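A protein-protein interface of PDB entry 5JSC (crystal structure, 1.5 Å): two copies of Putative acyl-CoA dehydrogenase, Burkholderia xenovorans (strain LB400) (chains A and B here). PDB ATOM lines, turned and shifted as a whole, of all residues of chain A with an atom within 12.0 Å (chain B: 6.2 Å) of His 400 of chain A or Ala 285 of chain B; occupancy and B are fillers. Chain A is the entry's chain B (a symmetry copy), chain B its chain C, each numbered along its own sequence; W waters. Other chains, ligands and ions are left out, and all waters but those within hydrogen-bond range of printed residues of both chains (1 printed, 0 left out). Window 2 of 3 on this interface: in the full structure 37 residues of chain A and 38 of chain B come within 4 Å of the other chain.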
ATOM      1  N   ARG A 333       2.494 -16.475   8.665  1.00  0.00           N
ATOM      2  CA  ARG A 333       3.184 -15.489   9.494  1.00  0.00           C
ATOM      3  C   ARG A 333       4.659 -15.388   9.137  1.00  0.00           C
ATOM      4  O   ARG A 333       5.196 -14.280   9.024  1.00  0.00           O
ATOM      5  CB  ARG A 333       3.036 -15.823  10.978  1.00  0.00           C
ATOM      6  CG  ARG A 333       3.551 -14.699  11.874  1.00  0.00           C
ATOM      7  CD  ARG A 333       3.643 -15.123  13.330  1.00  0.00           C
ATOM      8  NE  ARG A 333       2.349 -15.540  13.857  1.00  0.00           N
ATOM      9  CZ  ARG A 333       2.149 -15.941  15.106  1.00  0.00           C
ATOM     10  NH1 ARG A 333       3.160 -15.979  15.963  1.00  0.00           N
ATOM     11  NH2 ARG A 333       0.936 -16.309  15.492  1.00  0.00           N
ATOM     12  N   ILE A 391      -1.033  -8.705   8.179  1.00  0.00           N
ATOM     13  CA  ILE A 391      -1.083 -10.168   8.162  1.00  0.00           C
ATOM     14  C   ILE A 391      -0.492 -10.732   9.448  1.00  0.00           C
ATOM     15  O   ILE A 391      -1.086 -11.595  10.106  1.00  0.00           O
ATOM     16  CB  ILE A 391      -0.353 -10.718   6.922  1.00  0.00           C
ATOM     17  CG1 ILE A 391      -1.173 -10.458   5.657  1.00  0.00           C
ATOM     18  CG2 ILE A 391      -0.070 -12.212   7.073  1.00  0.00           C
ATOM     19  CD1 ILE A 391      -0.383 -10.672   4.369  1.00  0.00           C
ATOM     20  N   VAL A 392       0.694 -10.250   9.824  1.00  0.00           N
ATOM     21  CA  VAL A 392       1.342 -10.757  11.029  1.00  0.00           C
ATOM     22  C   VAL A 392       0.536 -10.381  12.266  1.00  0.00           C
ATOM     23  O   VAL A 392       0.282 -11.223  13.137  1.00  0.00           O
ATOM     24  CB  VAL A 392       2.789 -10.234  11.109  1.00  0.00           C
ATOM     25  CG1 VAL A 392       3.437 -10.625  12.436  1.00  0.00           C
ATOM     26  CG2 VAL A 392       3.601 -10.776   9.933  1.00  0.00           C
ATOM     27  N   GLY A 393       0.107  -9.120  12.357  1.00  0.00           N
ATOM     28  CA  GLY A 393      -0.645  -8.688  13.531  1.00  0.00           C
ATOM     29  C   GLY A 393      -1.946  -9.449  13.705  1.00  0.00           C
ATOM     30  O   GLY A 393      -2.285  -9.886  14.811  1.00  0.00           O
ATOM     31  N   ARG A 394      -2.705  -9.602  12.618  1.00  0.00           N
ATOM     32  CA  ARG A 394      -3.945 -10.370  12.708  1.00  0.00           C
ATOM     33  C   ARG A 394      -3.665 -11.812  13.104  1.00  0.00           C
ATOM     34  O   ARG A 394      -4.437 -12.416  13.860  1.00  0.00           O
ATOM     35  CB  ARG A 394      -4.705 -10.325  11.384  1.00  0.00           C
ATOM     36  CG  ARG A 394      -5.345  -8.981  11.053  1.00  0.00           C
ATOM     37  CD  ARG A 394      -6.423  -9.160   9.977  1.00  0.00           C
ATOM     38  NE  ARG A 394      -5.882  -9.697   8.727  1.00  0.00           N
ATOM     39  CZ  ARG A 394      -5.489  -8.946   7.699  1.00  0.00           C
ATOM     40  NH1 ARG A 394      -5.580  -7.621   7.766  1.00  0.00           N
ATOM     41  NH2 ARG A 394      -5.005  -9.517   6.603  1.00  0.00           N
ATOM     42  N   ASP A 395      -2.568 -12.388  12.600  1.00  0.00           N
ATOM     43  CA  ASP A 395      -2.286 -13.780  12.934  1.00  0.00           C
ATOM     44  C   ASP A 395      -1.924 -13.936  14.404  1.00  0.00           C
ATOM     45  O   ASP A 395      -2.278 -14.945  15.028  1.00  0.00           O
ATOM     46  CB  ASP A 395      -1.165 -14.334  12.052  1.00  0.00           C
ATOM     47  CG  ASP A 395      -1.022 -15.841  12.192  1.00  0.00           C
ATOM     48  OD1 ASP A 395      -1.954 -16.561  11.768  1.00  0.00           O
ATOM     49  OD2 ASP A 395       0.006 -16.311  12.732  1.00  0.00           O
ATOM     50  N   LEU A 396      -1.217 -12.953  14.975  1.00  0.00           N
ATOM     51  CA  LEU A 396      -0.921 -12.993  16.404  1.00  0.00           C
ATOM     52  C   LEU A 396      -2.198 -13.007  17.228  1.00  0.00           C
ATOM     53  O   LEU A 396      -2.308 -13.755  18.206  1.00  0.00           O
ATOM     54  CB  LEU A 396      -0.065 -11.795  16.803  1.00  0.00           C
ATOM     55  CG  LEU A 396       1.355 -11.784  16.253  1.00  0.00           C
ATOM     56  CD1 LEU A 396       1.932 -10.390  16.403  1.00  0.00           C
ATOM     57  CD2 LEU A 396       2.222 -12.823  16.973  1.00  0.00           C
ATOM     58  N   LEU A 397      -3.168 -12.165  16.858  1.00  0.00           N
ATOM     59  CA  LEU A 397      -4.421 -12.110  17.600  1.00  0.00           C
ATOM     60  C   LEU A 397      -5.250 -13.374  17.386  1.00  0.00           C
ATOM     61  O   LEU A 397      -5.905 -13.859  18.318  1.00  0.00           O
ATOM     62  CB  LEU A 397      -5.203 -10.865  17.183  1.00  0.00           C
ATOM     63  CG  LEU A 397      -4.549  -9.572  17.670  1.00  0.00           C
ATOM     64  CD1 LEU A 397      -5.051  -8.378  16.871  1.00  0.00           C
ATOM     65  CD2 LEU A 397      -4.805  -9.392  19.161  1.00  0.00           C
ATOM     66  N   LYS A 398      -5.221 -13.927  16.169  1.00  0.00           N
ATOM     67  CA  LYS A 398      -5.919 -15.180  15.896  1.00  0.00           C
ATOM     68  C   LYS A 398      -5.359 -16.310  16.748  1.00  0.00           C
ATOM     69  O   LYS A 398      -6.115 -17.094  17.337  1.00  0.00           O
ATOM     70  CB  LYS A 398      -5.810 -15.526  14.410  1.00  0.00           C
ATOM     71  CG  LYS A 398      -6.393 -16.880  14.028  1.00  0.00           C
ATOM     72  CD  LYS A 398      -6.118 -17.184  12.563  1.00  0.00           C
ATOM     73  CE  LYS A 398      -6.591 -18.581  12.189  1.00  0.00           C
ATOM     74  NZ  LYS A 398      -6.283 -18.928  10.772  1.00  0.00           N
ATOM     75  N   ALA A 399      -4.030 -16.407  16.827  1.00  0.00           N
ATOM     76  CA  ALA A 399      -3.421 -17.469  17.621  1.00  0.00           C
ATOM     77  C   ALA A 399      -3.728 -17.293  19.103  1.00  0.00           C
ATOM     78  O   ALA A 399      -3.961 -18.275  19.817  1.00  0.00           O
ATOM     79  CB  ALA A 399      -1.912 -17.506  17.379  1.00  0.00           C
ATOM     80  N   HIS A 400      -3.741 -16.047  19.584  1.00  0.00           N
ATOM     81  CA  HIS A 400      -4.085 -15.812  20.984  1.00  0.00           C
ATOM     82  C   HIS A 400      -5.524 -16.203  21.277  1.00  0.00           C
ATOM     83  O   HIS A 400      -5.811 -16.794  22.324  1.00  0.00           O
ATOM     84  CB  HIS A 400      -3.861 -14.343  21.347  1.00  0.00           C
ATOM     85  CG  HIS A 400      -4.152 -14.040  22.782  1.00  0.00           C
ATOM     86  ND1 HIS A 400      -5.229 -13.278  23.183  1.00  0.00           N
ATOM     87  CD2 HIS A 400      -3.528 -14.436  23.917  1.00  0.00           C
ATOM     88  CE1 HIS A 400      -5.244 -13.198  24.502  1.00  0.00           C
ATOM     89  NE2 HIS A 400      -4.225 -13.896  24.972  1.00  0.00           N
ATOM     90  N   ALA A 401      -6.443 -15.868  20.370  1.00  0.00           N
ATOM     91  CA  ALA A 401      -7.837 -16.263  20.553  1.00  0.00           C
ATOM     92  C   ALA A 401      -7.975 -17.777  20.604  1.00  0.00           C
ATOM     93  O   ALA A 401      -8.733 -18.314  21.421  1.00  0.00           O
ATOM     94  CB  ALA A 401      -8.694 -15.684  19.427  1.00  0.00           C
ATOM     95  N   ALA A 402      -7.243 -18.483  19.741  1.00  0.00           N
ATOM     96  CA  ALA A 402      -7.320 -19.941  19.729  1.00  0.00           C
ATOM     97  C   ALA A 402      -6.777 -20.527  21.025  1.00  0.00           C
ATOM     98  O   ALA A 402      -7.309 -21.521  21.537  1.00  0.00           O
ATOM     99  CB  ALA A 402      -6.557 -20.487  18.526  1.00  0.00           C
ATOM    100  N   ALA A 403      -5.719 -19.922  21.571  1.00  0.00           N
ATOM    101  CA  ALA A 403      -5.113 -20.427  22.797  1.00  0.00           C
ATOM    102  C   ALA A 403      -6.030 -20.219  23.995  1.00  0.00           C
ATOM    103  O   ALA A 403      -6.114 -21.082  24.878  1.00  0.00           O
ATOM    104  CB  ALA A 403      -3.763 -19.748  23.028  1.00  0.00           C
ATOM    105  N   THR A 404      -6.726 -19.086  24.042  1.00  0.00           N
ATOM    106  CA  THR A 404      -7.622 -18.776  25.148  1.00  0.00           C
ATOM    107  C   THR A 404      -9.005 -19.387  24.974  1.00  0.00           C
ATOM    108  O   THR A 404      -9.855 -19.217  25.856  1.00  0.00           O
ATOM    109  CB  THR A 404      -7.743 -17.258  25.320  1.00  0.00           C
ATOM    110  OG1 THR A 404      -8.319 -16.683  24.140  1.00  0.00           O
ATOM    111  CG2 THR A 404      -6.374 -16.640  25.559  1.00  0.00           C
ATOM    112  N   ALA A 405      -9.250 -20.083  23.869  1.00  0.00           N
ATOM    113  CA  ALA A 405     -10.497 -20.810  23.678  1.00  0.00           C
ATOM    114  C   ALA A 405     -10.372 -22.212  24.258  1.00  0.00           C
ATOM    115  O   ALA A 405      -9.301 -22.821  24.201  1.00  0.00           O
ATOM    116  CB  ALA A 405     -10.861 -20.872  22.205  1.00  0.00           C
ATOM    117  N   ALA B 278       3.545 -11.397  25.435  1.00  0.00           N
ATOM    118  CA  ALA B 278       2.344 -12.038  25.964  1.00  0.00           C
ATOM    119  C   ALA B 278       1.430 -11.020  26.633  1.00  0.00           C
ATOM    120  O   ALA B 278       0.209 -11.041  26.430  1.00  0.00           O
ATOM    121  CB  ALA B 278       2.736 -13.154  26.938  1.00  0.00           C
ATOM    122  N   GLY B 280       1.268  -7.817  25.978  1.00  0.00           N
ATOM    123  CA  GLY B 280       0.751  -6.891  24.982  1.00  0.00           C
ATOM    124  C   GLY B 280      -0.375  -7.482  24.153  1.00  0.00           C
ATOM    125  O   GLY B 280      -1.398  -6.829  23.928  1.00  0.00           O
ATOM    126  N   VAL B 281      -0.209  -8.724  23.680  1.00  0.00           N
ATOM    127  CA  VAL B 281      -1.273  -9.308  22.874  1.00  0.00           C
ATOM    128  C   VAL B 281      -2.515  -9.556  23.728  1.00  0.00           C
ATOM    129  O   VAL B 281      -3.641  -9.338  23.265  1.00  0.00           O
ATOM    130  CB  VAL B 281      -0.777 -10.576  22.140  1.00  0.00           C
ATOM    131  CG1 VAL B 281      -0.600 -11.774  23.081  1.00  0.00           C
ATOM    132  CG2 VAL B 281      -1.707 -10.920  20.970  1.00  0.00           C
ATOM    133  N   ALA B 282      -2.339  -9.979  24.986  1.00  0.00           N
ATOM    134  CA  ALA B 282      -3.500 -10.179  25.847  1.00  0.00           C
ATOM    135  C   ALA B 282      -4.247  -8.872  26.088  1.00  0.00           C
ATOM    136  O   ALA B 282      -5.482  -8.852  26.102  1.00  0.00           O
ATOM    137  CB  ALA B 282      -3.073 -10.801  27.172  1.00  0.00           C
ATOM    138  N   ARG B 283      -3.515  -7.773  26.292  1.00  0.00           N
ATOM    139  CA  ARG B 283      -4.164  -6.487  26.534  1.00  0.00           C
ATOM    140  C   ARG B 283      -4.843  -5.967  25.275  1.00  0.00           C
ATOM    141  O   ARG B 283      -5.955  -5.429  25.343  1.00  0.00           O
ATOM    142  CB  ARG B 283      -3.141  -5.480  27.056  1.00  0.00           C
ATOM    143  CG  ARG B 283      -3.739  -4.127  27.430  1.00  0.00           C
ATOM    144  CD  ARG B 283      -4.669  -4.248  28.636  1.00  0.00           C
ATOM    145  NE  ARG B 283      -5.019  -2.917  29.133  1.00  0.00           N
ATOM    146  CZ  ARG B 283      -5.507  -2.660  30.342  1.00  0.00           C
ATOM    147  NH1 ARG B 283      -5.724  -3.648  31.205  1.00  0.00           N
ATOM    148  NH2 ARG B 283      -5.765  -1.403  30.691  1.00  0.00           N
ATOM    149  N   ALA B 284      -4.207  -6.153  24.113  1.00  0.00           N
ATOM    150  CA  ALA B 284      -4.834  -5.768  22.853  1.00  0.00           C
ATOM    151  C   ALA B 284      -6.160  -6.497  22.656  1.00  0.00           C
ATOM    152  O   ALA B 284      -7.154  -5.903  22.220  1.00  0.00           O
ATOM    153  CB  ALA B 284      -3.879  -6.054  21.688  1.00  0.00           C
ATOM    154  N   ALA B 285      -6.197  -7.784  22.997  1.00  0.00           N
ATOM    155  CA  ALA B 285      -7.401  -8.580  22.795  1.00  0.00           C
ATOM    156  C   ALA B 285      -8.495  -8.236  23.796  1.00  0.00           C
ATOM    157  O   ALA B 285      -9.684  -8.333  23.465  1.00  0.00           O
ATOM    158  CB  ALA B 285      -7.059 -10.066  22.888  1.00  0.00           C
ATOM    159  N   SER B 286      -8.127  -7.846  25.015  1.00  0.00           N
ATOM    160  CA  SER B 286      -9.101  -7.692  26.087  1.00  0.00           C
ATOM    161  C   SER B 286      -9.562  -6.258  26.315  1.00  0.00           C
ATOM    162  O   SER B 286     -10.652  -6.071  26.867  1.00  0.00           O
ATOM    163  CB  SER B 286      -8.540  -8.237  27.405  1.00  0.00           C
ATOM    164  OG  SER B 286      -7.449  -7.455  27.858  1.00  0.00           O
ATOM    165  N   ARG B 287      -8.785  -5.249  25.912  1.00  0.00           N
ATOM    166  CA  ARG B 287      -9.099  -3.863  26.259  1.00  0.00           C
ATOM    167  C   ARG B 287     -10.165  -3.316  25.317  1.00  0.00           C
ATOM    168  O   ARG B 287      -9.903  -3.089  24.132  1.00  0.00           O
ATOM    169  CB  ARG B 287      -7.842  -2.999  26.210  1.00  0.00           C
ATOM    170  CG  ARG B 287      -8.072  -1.549  26.629  1.00  0.00           C
ATOM    171  CD  ARG B 287      -8.514  -1.448  28.082  1.00  0.00           C
ATOM    172  NE  ARG B 287      -8.426  -0.070  28.585  1.00  0.00           N
ATOM    173  CZ  ARG B 287      -8.820   0.308  29.797  1.00  0.00           C
ATOM    174  NH1 ARG B 287      -9.338  -0.588  30.627  1.00  0.00           N
ATOM    175  NH2 ARG B 287      -8.694   1.576  30.183  1.00  0.00           N
ATOM    176  N   LYS B 288     -11.363  -3.083  25.847  1.00  0.00           N
ATOM    177  CA  LYS B 288     -12.449  -2.524  25.053  1.00  0.00           C
ATOM    178  C   LYS B 288     -12.288  -1.012  24.925  1.00  0.00           C
ATOM    179  O   LYS B 288     -11.969  -0.322  25.898  1.00  0.00           O
ATOM    180  CB  LYS B 288     -13.796  -2.850  25.695  1.00  0.00           C
ATOM    181  CG  LYS B 288     -14.091  -4.337  25.796  1.00  0.00           C
ATOM    182  CD  LYS B 288     -15.470  -4.572  26.454  1.00  0.00           C
ATOM    183  CE  LYS B 288     -15.770  -6.044  26.654  1.00  0.00           C
ATOM    184  NZ  LYS B 288     -14.966  -6.630  27.759  1.00  0.00           N
ATOM    185  N   THR B 293     -12.142  -3.481  20.279  1.00  0.00           N
ATOM    186  CA  THR B 293     -11.022  -3.707  21.182  1.00  0.00           C
ATOM    187  C   THR B 293      -9.791  -3.007  20.634  1.00  0.00           C
ATOM    188  O   THR B 293      -9.717  -2.681  19.445  1.00  0.00           O
ATOM    189  CB  THR B 293     -10.697  -5.196  21.380  1.00  0.00           C
ATOM    190  OG1 THR B 293     -10.238  -5.749  20.139  1.00  0.00           O
ATOM    191  CG2 THR B 293     -11.910  -5.965  21.881  1.00  0.00           C
ATOM    192  N   LEU B 294      -8.829  -2.774  21.531  1.00  0.00           N
ATOM    193  CA  LEU B 294      -7.564  -2.161  21.142  1.00  0.00           C
ATOM    194  C   LEU B 294      -6.921  -2.913  19.976  1.00  0.00           C
ATOM    195  O   LEU B 294      -6.370  -2.300  19.049  1.00  0.00           O
ATOM    196  CB  LEU B 294      -6.642  -2.118  22.364  1.00  0.00           C
ATOM    197  CG  LEU B 294      -5.208  -1.598  22.216  1.00  0.00           C
ATOM    198  CD1 LEU B 294      -5.203  -0.180  21.641  1.00  0.00           C
ATOM    199  CD2 LEU B 294      -4.508  -1.636  23.568  1.00  0.00           C
ATOM    200  N   GLY B 295      -7.004  -4.246  19.990  1.00  0.00           N
ATOM    201  CA  GLY B 295      -6.408  -5.050  18.936  1.00  0.00           C
ATOM    202  C   GLY B 295      -7.079  -4.934  17.581  1.00  0.00           C
ATOM    203  O   GLY B 295      -6.501  -5.372  16.583  1.00  0.00           O
HETATM  204  O   HOH W   1      -0.902 -13.517  25.960  1.00  0.00           O
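Among the printed residues, merely in contact across the chains: Leu 397 of chain A with Gly 295 of chain B (3.3 Å), His 400 of chain A with Ala 285 of chain B (3.7 Å), His 400 of chain A with Ala 282 of chain B (3.7 Å) and Leu 397 of chain A with Val 281 of chain B (3.9 Å).
Of the printed residues of chain B, His 400 of chain A touches Ala 282 and Ala 285.
Of chain A, only His 400 comes within 4 Å of Ala 285 of chain B.
No residue of chain A comes within 4 Å of Ala 278 of chain B.
Ala 282 of chain B touches just one residue of chain A: His 400.
Ala 284 of chain B touches none of the printed residues of chain A.
No residue of chain A comes within 4 Å of Ser 286 of chain B.
No residue of chain A comes within 4 Å of Thr 293 of chain B.
No residue of chain A comes within 4 Å of Leu 294 of chain B.
Of the printed residues of chain A, Gly 295 of chain B touches Leu 397.
Of the printed residues of chain A, Val 281 of chain B touches Leu 397 (3.9 Å).
Printed residues of chain B within 4 Å of Leu 397 of chain A: Val 281 (3.9 Å) and Gly 295 (3.3 Å).
Ala 399 of chain A touches none of the printed residues of chain B.
The nearest residue of chain A that does not touch Ala 285 of chain B is Leu 397 of chain A (4.4 Å).
No position is printed for both chains.
Of the 16 printed residues of chain A, 2 touch a printed residue of chain B.
Hydrophobic or aromatic side chains of chain A that line the printed part of chain B: Leu 397 and His 400.
Of the 13 printed residues of chain B, 4 touch a printed residue of chain A.
Printed residues of chain B that touch a printed residue of chain A: Val 281, Ala 282, Ala 285 and Gly 295.
Among the printed residues, 4 pairs touch across the chains.
Among the printed residues, no Asp or Glu carboxylate lies within 4 Å of a Lys or Arg side-chain nitrogen of the other chain.
Water W1 bridges O of Ala 278 of chain B and NE2 of His 400 of chain A.
The backbone carbonyl oxygen (O) of Ala 282 of chain B lies within hydrogen-bond range of the side-chain hydroxyl (OG) of Ser 286 of chain B (3.0 Å).
N of Gly 295 of chain B is in hydrogen-bond range of O of Ala 284 of chain B, at 2.8 Å.
The side-chain hydroxyl (OG1) of Thr 404 of chain A is in hydrogen-bond range of the backbone carbonyl oxygen (O) of His 400 of chain A, 3.1 Å away.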
